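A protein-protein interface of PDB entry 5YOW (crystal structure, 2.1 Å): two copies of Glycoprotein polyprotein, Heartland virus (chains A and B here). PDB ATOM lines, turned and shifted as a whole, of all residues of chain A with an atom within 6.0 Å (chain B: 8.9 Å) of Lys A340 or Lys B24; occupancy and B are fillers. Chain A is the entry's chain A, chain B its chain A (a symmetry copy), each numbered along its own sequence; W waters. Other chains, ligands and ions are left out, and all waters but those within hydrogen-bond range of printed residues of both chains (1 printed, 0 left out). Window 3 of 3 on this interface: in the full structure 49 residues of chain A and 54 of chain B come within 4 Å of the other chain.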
ATOM      1  N   CYS A  44     -11.929   5.521   4.358  1.00  0.00           N
ATOM      2  CA  CYS A  44     -12.436   4.497   5.271  1.00  0.00           C
ATOM      3  C   CYS A  44     -13.175   5.205   6.401  1.00  0.00           C
ATOM      4  O   CYS A  44     -12.562   5.938   7.183  1.00  0.00           O
ATOM      5  CB  CYS A  44     -11.305   3.598   5.795  1.00  0.00           C
ATOM      6  SG  CYS A  44     -11.655   2.597   7.292  1.00  0.00           S
ATOM      7  N   LEU A  45     -14.491   5.012   6.461  1.00  0.00           N
ATOM      8  CA  LEU A  45     -15.365   5.736   7.378  1.00  0.00           C
ATOM      9  C   LEU A  45     -15.942   4.752   8.382  1.00  0.00           C
ATOM     10  O   LEU A  45     -16.601   3.783   7.992  1.00  0.00           O
ATOM     11  CB  LEU A  45     -16.497   6.441   6.627  1.00  0.00           C
ATOM     12  CG  LEU A  45     -16.187   7.816   6.019  1.00  0.00           C
ATOM     13  CD1 LEU A  45     -15.287   7.679   4.791  1.00  0.00           C
ATOM     14  CD2 LEU A  45     -17.479   8.563   5.661  1.00  0.00           C
ATOM     15  N   HIS A  46     -15.704   5.005   9.667  1.00  0.00           N
ATOM     16  CA  HIS A  46     -16.144   4.114  10.730  1.00  0.00           C
ATOM     17  C   HIS A  46     -17.341   4.742  11.427  1.00  0.00           C
ATOM     18  O   HIS A  46     -17.257   5.872  11.905  1.00  0.00           O
ATOM     19  CB  HIS A  46     -15.023   3.864  11.734  1.00  0.00           C
ATOM     20  CG  HIS A  46     -14.040   2.827  11.301  1.00  0.00           C
ATOM     21  ND1 HIS A  46     -14.322   1.476  11.323  1.00  0.00           N
ATOM     22  CD2 HIS A  46     -12.766   2.940  10.858  1.00  0.00           C
ATOM     23  CE1 HIS A  46     -13.267   0.803  10.898  1.00  0.00           C
ATOM     24  NE2 HIS A  46     -12.308   1.668  10.614  1.00  0.00           N
ATOM     25  N   PHE A  47     -18.450   4.013  11.467  1.00  0.00           N
ATOM     26  CA  PHE A  47     -19.672   4.474  12.105  1.00  0.00           C
ATOM     27  C   PHE A  47     -19.905   3.657  13.364  1.00  0.00           C
ATOM     28  O   PHE A  47     -19.808   2.428  13.336  1.00  0.00           O
ATOM     29  CB  PHE A  47     -20.864   4.349  11.159  1.00  0.00           C
ATOM     30  CG  PHE A  47     -20.724   5.172   9.914  1.00  0.00           C
ATOM     31  CD1 PHE A  47     -20.952   6.535   9.949  1.00  0.00           C
ATOM     32  CD2 PHE A  47     -20.323   4.594   8.714  1.00  0.00           C
ATOM     33  CE1 PHE A  47     -20.814   7.303   8.798  1.00  0.00           C
ATOM     34  CE2 PHE A  47     -20.189   5.355   7.557  1.00  0.00           C
ATOM     35  CZ  PHE A  47     -20.447   6.712   7.599  1.00  0.00           C
ATOM     36  N   SER A  48     -20.195   4.334  14.465  1.00  0.00           N
ATOM     37  CA  SER A  48     -20.512   3.661  15.715  1.00  0.00           C
ATOM     38  C   SER A  48     -21.772   4.275  16.288  1.00  0.00           C
ATOM     39  O   SER A  48     -21.907   5.500  16.336  1.00  0.00           O
ATOM     40  CB  SER A  48     -19.366   3.761  16.732  1.00  0.00           C
ATOM     41  OG  SER A  48     -18.885   5.091  16.868  1.00  0.00           O
ATOM     42  N   ASP A  54     -18.040  -0.949  17.110  1.00  0.00           N
ATOM     43  CA  ASP A  54     -17.721  -0.157  15.932  1.00  0.00           C
ATOM     44  C   ASP A  54     -17.750  -1.037  14.692  1.00  0.00           C
ATOM     45  O   ASP A  54     -17.186  -2.138  14.682  1.00  0.00           O
ATOM     46  CB  ASP A  54     -16.360   0.535  16.079  1.00  0.00           C
ATOM     47  CG  ASP A  54     -16.284   1.837  15.294  1.00  0.00           C
ATOM     48  OD1 ASP A  54     -16.901   1.908  14.209  1.00  0.00           O
ATOM     49  OD2 ASP A  54     -15.617   2.789  15.761  1.00  0.00           O
ATOM     50  N   ARG A 338     -22.050   8.153  15.243  1.00  0.00           N
ATOM     51  CA  ARG A 338     -20.821   8.927  15.264  1.00  0.00           C
ATOM     52  C   ARG A 338     -19.890   8.388  14.190  1.00  0.00           C
ATOM     53  O   ARG A 338     -19.892   7.193  13.880  1.00  0.00           O
ATOM     54  CB  ARG A 338     -20.127   8.856  16.629  1.00  0.00           C
ATOM     55  CG  ARG A 338     -20.896   9.483  17.788  1.00  0.00           C
ATOM     56  CD  ARG A 338     -20.296   9.088  19.146  1.00  0.00           C
ATOM     57  NE  ARG A 338     -19.020   9.750  19.426  1.00  0.00           N
ATOM     58  CZ  ARG A 338     -17.838   9.135  19.450  1.00  0.00           C
ATOM     59  NH1 ARG A 338     -17.752   7.831  19.207  1.00  0.00           N
ATOM     60  NH2 ARG A 338     -16.735   9.827  19.718  1.00  0.00           N
ATOM     61  N   LEU A 339     -19.081   9.279  13.640  1.00  0.00           N
ATOM     62  CA  LEU A 339     -18.141   8.954  12.582  1.00  0.00           C
ATOM     63  C   LEU A 339     -16.716   9.077  13.106  1.00  0.00           C
ATOM     64  O   LEU A 339     -16.368  10.052  13.783  1.00  0.00           O
ATOM     65  CB  LEU A 339     -18.322   9.889  11.373  1.00  0.00           C
ATOM     66  CG  LEU A 339     -17.197   9.919  10.322  1.00  0.00           C
ATOM     67  CD1 LEU A 339     -17.027   8.536   9.675  1.00  0.00           C
ATOM     68  CD2 LEU A 339     -17.439  10.988   9.224  1.00  0.00           C
ATOM     69  N   LYS A 340     -15.888   8.120  12.731  1.00  0.00           N
ATOM     70  CA  LYS A 340     -14.451   8.194  12.932  1.00  0.00           C
ATOM     71  C   LYS A 340     -13.780   7.893  11.604  1.00  0.00           C
ATOM     72  O   LYS A 340     -14.209   6.985  10.885  1.00  0.00           O
ATOM     73  CB  LYS A 340     -13.984   7.178  13.979  1.00  0.00           C
ATOM     74  CG  LYS A 340     -14.530   7.425  15.367  1.00  0.00           C
ATOM     75  CD  LYS A 340     -14.046   6.356  16.343  1.00  0.00           C
ATOM     76  CE  LYS A 340     -14.516   6.661  17.761  1.00  0.00           C
ATOM     77  NZ  LYS A 340     -14.417   5.464  18.643  1.00  0.00           N
ATOM     78  N   LEU A 341     -12.722   8.642  11.287  1.00  0.00           N
ATOM     79  CA  LEU A 341     -11.975   8.467  10.044  1.00  0.00           C
ATOM     80  C   LEU A 341     -10.708   7.672  10.310  1.00  0.00           C
ATOM     81  O   LEU A 341      -9.973   7.977  11.247  1.00  0.00           O
ATOM     82  CB  LEU A 341     -11.603   9.821   9.440  1.00  0.00           C
ATOM     83  CG  LEU A 341     -12.709  10.878   9.378  1.00  0.00           C
ATOM     84  CD1 LEU A 341     -12.162  12.254   9.013  1.00  0.00           C
ATOM     85  CD2 LEU A 341     -13.757  10.448   8.367  1.00  0.00           C
ATOM     86  N   SER A 342     -10.435   6.670   9.477  1.00  0.00           N
ATOM     87  CA  SER A 342      -9.152   5.969   9.501  1.00  0.00           C
ATOM     88  C   SER A 342      -8.262   6.556   8.416  1.00  0.00           C
ATOM     89  O   SER A 342      -8.607   6.501   7.229  1.00  0.00           O
ATOM     90  CB  SER A 342      -9.327   4.468   9.289  1.00  0.00           C
ATOM     91  OG  SER A 342      -9.867   3.871  10.440  1.00  0.00           O
ATOM     92  N   LYS B  12     -14.611  19.477  12.950  1.00  0.00           N
ATOM     93  CA  LYS B  12     -13.814  18.810  13.985  1.00  0.00           C
ATOM     94  C   LYS B  12     -14.136  17.331  13.825  1.00  0.00           C
ATOM     95  O   LYS B  12     -15.247  16.898  14.132  1.00  0.00           O
ATOM     96  CB  LYS B  12     -14.173  19.346  15.369  1.00  0.00           C
ATOM     97  CG  LYS B  12     -13.686  18.551  16.571  1.00  0.00           C
ATOM     98  CD  LYS B  12     -14.614  17.392  16.986  1.00  0.00           C
ATOM     99  CE  LYS B  12     -14.339  16.836  18.373  1.00  0.00           C
ATOM    100  NZ  LYS B  12     -14.944  15.473  18.468  1.00  0.00           N
ATOM    101  N   SER B  13     -13.219  16.569  13.260  1.00  0.00           N
ATOM    102  CA  SER B  13     -13.446  15.146  13.105  1.00  0.00           C
ATOM    103  C   SER B  13     -12.485  14.381  13.994  1.00  0.00           C
ATOM    104  O   SER B  13     -11.427  14.881  14.377  1.00  0.00           O
ATOM    105  CB  SER B  13     -13.269  14.709  11.654  1.00  0.00           C
ATOM    106  OG  SER B  13     -14.210  15.360  10.821  1.00  0.00           O
ATOM    107  N   ILE B  14     -12.862  13.150  14.293  1.00  0.00           N
ATOM    108  CA  ILE B  14     -12.008  12.199  14.977  1.00  0.00           C
ATOM    109  C   ILE B  14     -11.295  11.379  13.917  1.00  0.00           C
ATOM    110  O   ILE B  14     -11.934  10.741  13.077  1.00  0.00           O
ATOM    111  CB  ILE B  14     -12.820  11.305  15.921  1.00  0.00           C
ATOM    112  CG1 ILE B  14     -13.392  12.151  17.058  1.00  0.00           C
ATOM    113  CG2 ILE B  14     -11.947  10.176  16.476  1.00  0.00           C
ATOM    114  CD1 ILE B  14     -14.511  11.478  17.779  1.00  0.00           C
ATOM    115  N   THR B  15      -9.974  11.399  13.935  1.00  0.00           N
ATOM    116  CA  THR B  15      -9.194  10.616  12.994  1.00  0.00           C
ATOM    117  C   THR B  15      -8.317   9.638  13.766  1.00  0.00           C
ATOM    118  O   THR B  15      -7.797   9.967  14.834  1.00  0.00           O
ATOM    119  CB  THR B  15      -8.352  11.517  12.082  1.00  0.00           C
ATOM    120  OG1 THR B  15      -7.626  10.702  11.163  1.00  0.00           O
ATOM    121  CG2 THR B  15      -7.388  12.368  12.880  1.00  0.00           C
ATOM    122  N   CYS B  16      -8.175   8.437  13.214  1.00  0.00           N
ATOM    123  CA  CYS B  16      -7.575   7.300  13.889  1.00  0.00           C
ATOM    124  C   CYS B  16      -6.461   6.702  13.044  1.00  0.00           C
ATOM    125  O   CYS B  16      -6.524   6.691  11.815  1.00  0.00           O
ATOM    126  CB  CYS B  16      -8.619   6.202  14.187  1.00  0.00           C
ATOM    127  SG  CYS B  16     -10.031   6.732  15.182  1.00  0.00           S
ATOM    128  N   LYS B  17      -5.452   6.182  13.732  1.00  0.00           N
ATOM    129  CA  LYS B  17      -4.342   5.459  13.134  1.00  0.00           C
ATOM    130  C   LYS B  17      -4.428   3.998  13.551  1.00  0.00           C
ATOM    131  O   LYS B  17      -4.666   3.698  14.727  1.00  0.00           O
ATOM    132  CB  LYS B  17      -3.007   6.053  13.585  1.00  0.00           C
ATOM    133  CG  LYS B  17      -2.524   7.185  12.717  1.00  0.00           C
ATOM    134  CD  LYS B  17      -1.923   8.285  13.558  1.00  0.00           C
ATOM    135  CE  LYS B  17      -1.524   9.482  12.694  1.00  0.00           C
ATOM    136  NZ  LYS B  17      -0.900  10.553  13.529  1.00  0.00           N
ATOM    137  N   SER B  18      -4.246   3.101  12.585  1.00  0.00           N
ATOM    138  CA  SER B  18      -4.267   1.650  12.815  1.00  0.00           C
ATOM    139  C   SER B  18      -5.419   1.199  13.717  1.00  0.00           C
ATOM    140  O   SER B  18      -5.205   0.743  14.843  1.00  0.00           O
ATOM    141  CB  SER B  18      -2.928   1.182  13.407  1.00  0.00           C
ATOM    142  OG  SER B  18      -1.927   1.098  12.404  1.00  0.00           O
ATOM    143  N   GLU B  23      -4.829  -2.086  18.913  1.00  0.00           N
ATOM    144  CA  GLU B  23      -5.915  -1.180  19.279  1.00  0.00           C
ATOM    145  C   GLU B  23      -6.132  -0.082  18.227  1.00  0.00           C
ATOM    146  O   GLU B  23      -6.450  -0.368  17.070  1.00  0.00           O
ATOM    147  CB  GLU B  23      -5.640  -0.547  20.650  1.00  0.00           C
ATOM    148  CG  GLU B  23      -6.884  -0.057  21.381  1.00  0.00           C
ATOM    149  CD  GLU B  23      -6.551   0.880  22.523  1.00  0.00           C
ATOM    150  OE1 GLU B  23      -5.866   0.446  23.474  1.00  0.00           O
ATOM    151  OE2 GLU B  23      -6.963   2.058  22.463  1.00  0.00           O
ATOM    152  N   LYS B  24      -5.948   1.169  18.644  1.00  0.00           N
ATOM    153  CA  LYS B  24      -6.239   2.344  17.836  1.00  0.00           C
ATOM    154  C   LYS B  24      -5.715   3.577  18.560  1.00  0.00           C
ATOM    155  O   LYS B  24      -5.653   3.612  19.794  1.00  0.00           O
ATOM    156  CB  LYS B  24      -7.743   2.488  17.578  1.00  0.00           C
ATOM    157  CG  LYS B  24      -8.515   2.845  18.834  1.00  0.00           C
ATOM    158  CD  LYS B  24     -10.005   2.888  18.613  1.00  0.00           C
ATOM    159  CE  LYS B  24     -10.654   3.763  19.666  1.00  0.00           C
ATOM    160  NZ  LYS B  24     -11.946   4.302  19.189  1.00  0.00           N
ATOM    161  N   GLU B  25      -5.344   4.584  17.782  1.00  0.00           N
ATOM    162  CA  GLU B  25      -4.897   5.873  18.302  1.00  0.00           C
ATOM    163  C   GLU B  25      -5.772   6.922  17.622  1.00  0.00           C
ATOM    164  O   GLU B  25      -5.566   7.210  16.441  1.00  0.00           O
ATOM    165  CB  GLU B  25      -3.419   6.103  17.998  1.00  0.00           C
ATOM    166  CG  GLU B  25      -2.459   5.655  19.078  1.00  0.00           C
ATOM    167  CD  GLU B  25      -1.951   6.823  19.911  1.00  0.00           C
ATOM    168  OE1 GLU B  25      -2.274   7.990  19.577  1.00  0.00           O
ATOM    169  OE2 GLU B  25      -1.234   6.569  20.906  1.00  0.00           O
ATOM    170  N   CYS B  26      -6.754   7.466  18.341  1.00  0.00           N
ATOM    171  CA  CYS B  26      -7.722   8.393  17.766  1.00  0.00           C
ATOM    172  C   CYS B  26      -7.571   9.764  18.412  1.00  0.00           C
ATOM    173  O   CYS B  26      -7.402   9.866  19.624  1.00  0.00           O
ATOM    174  CB  CYS B  26      -9.168   7.901  17.955  1.00  0.00           C
ATOM    175  SG  CYS B  26      -9.589   6.331  17.151  1.00  0.00           S
ATOM    176  N   SER B  27      -7.650  10.816  17.597  1.00  0.00           N
ATOM    177  CA  SER B  27      -7.566  12.180  18.103  1.00  0.00           C
ATOM    178  C   SER B  27      -8.413  13.101  17.232  1.00  0.00           C
ATOM    179  O   SER B  27      -8.886  12.727  16.155  1.00  0.00           O
ATOM    180  CB  SER B  27      -6.111  12.682  18.163  1.00  0.00           C
ATOM    181  OG  SER B  27      -5.400  12.361  16.975  1.00  0.00           O
HETATM  182  O   HOH W   1     -15.945  12.437  13.687  1.00  0.00           O
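No residue of chain B comes within 4 Å of Leu A339. Lys A340 touches two residues of chain B. Of the printed residues of chain A, Ser B13 touches Leu A341 (3.8 Å). Of the printed residues of chain A, Thr B15 touches Leu A341 (3.3 Å). Ser B27 touches none of the printed residues of chain A. The nearest residue of chain B that does not touch Lys A340 is Cys B16 (4.2 Å). The nearest residue of chain A that does not touch Lys B24 is Asp A54 (5.2 Å).
Printed residues of chain A that touch a printed residue of chain B: Arg A338, Lys A340, Leu A341 and Ser A342. Of the 12 printed residues of chain B, 5 touch a printed residue of chain A. Printed residues of chain B that touch a printed residue of chain A: Ser B13, Ile B14, Thr B15, Cys B16 and Lys B24. Hydrophobic or aromatic side chains of chain B that line the printed part of chain A: Ile B14. Along chain B the printed residues that touch a printed residue of chain A span positions 13 to 24. Among the printed residues, 8 pairs touch across the chains. Among the printed residues, no Asp or Glu carboxylate lies within 4 Å of a Lys or Arg side-chain nitrogen of the other chain.
Water W1 lies within hydrogen-bond range of O of Leu A339 (2.4 Å) and N of Ile B14 (3.2 Å).
No position is printed for both chains. Of the 8 pairs that touch across the chains among the printed residues, none has its exchanged pair printed and touching as well.
The backbone NH (N) of Leu A341 is in hydrogen-bond range of the backbone carbonyl oxygen (O) of Ile B14 (2.9 Å). The backbone NH of Cys B16 sits at hydrogen-bond distance from the backbone carbonyl oxygen of Leu A341 (2.7 Å). NZ of Lys A340 sits close to NZ of Lys B24 (2.8 Å).
CD1 of Ile B14 touches NH2 of Arg A338, 3.4 Å away. Lys A340 touches Ile B14 (CA to O, 3.6 Å). Ser B13 touches Leu A341 (CB to CD1, 3.8 Å). O of Leu A341 touches CA of Thr B15, at 3.3 Å. O of Cys B16 touches CA of Ser A342 (3.6 Å).
O of Cys A44 sits at hydrogen-bond distance from N of Ser A342 (3.2 Å). O of His A46 lies within hydrogen-bond range of N of Lys A340, 2.8 Å away. A ring nitrogen (NE2) of His A46 lies close to the side-chain hydroxyl (OG) of Ser A342 (3.3 Å). The backbone NH (N) of Arg A338 sits at hydrogen-bond distance from the backbone carbonyl oxygen (O) of Ser A48 (2.9 Å). The side-chain sulfur (SG) of Cys B26 is disulfide-bonded to the side-chain sulfur (SG) of Cys B16, 2.1 Å away. The side-chain sulfur (SG) of Cys B26 is in hydrogen-bond range of the side-chain amino group (NZ) of Lys B24, at 3.7 Å.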
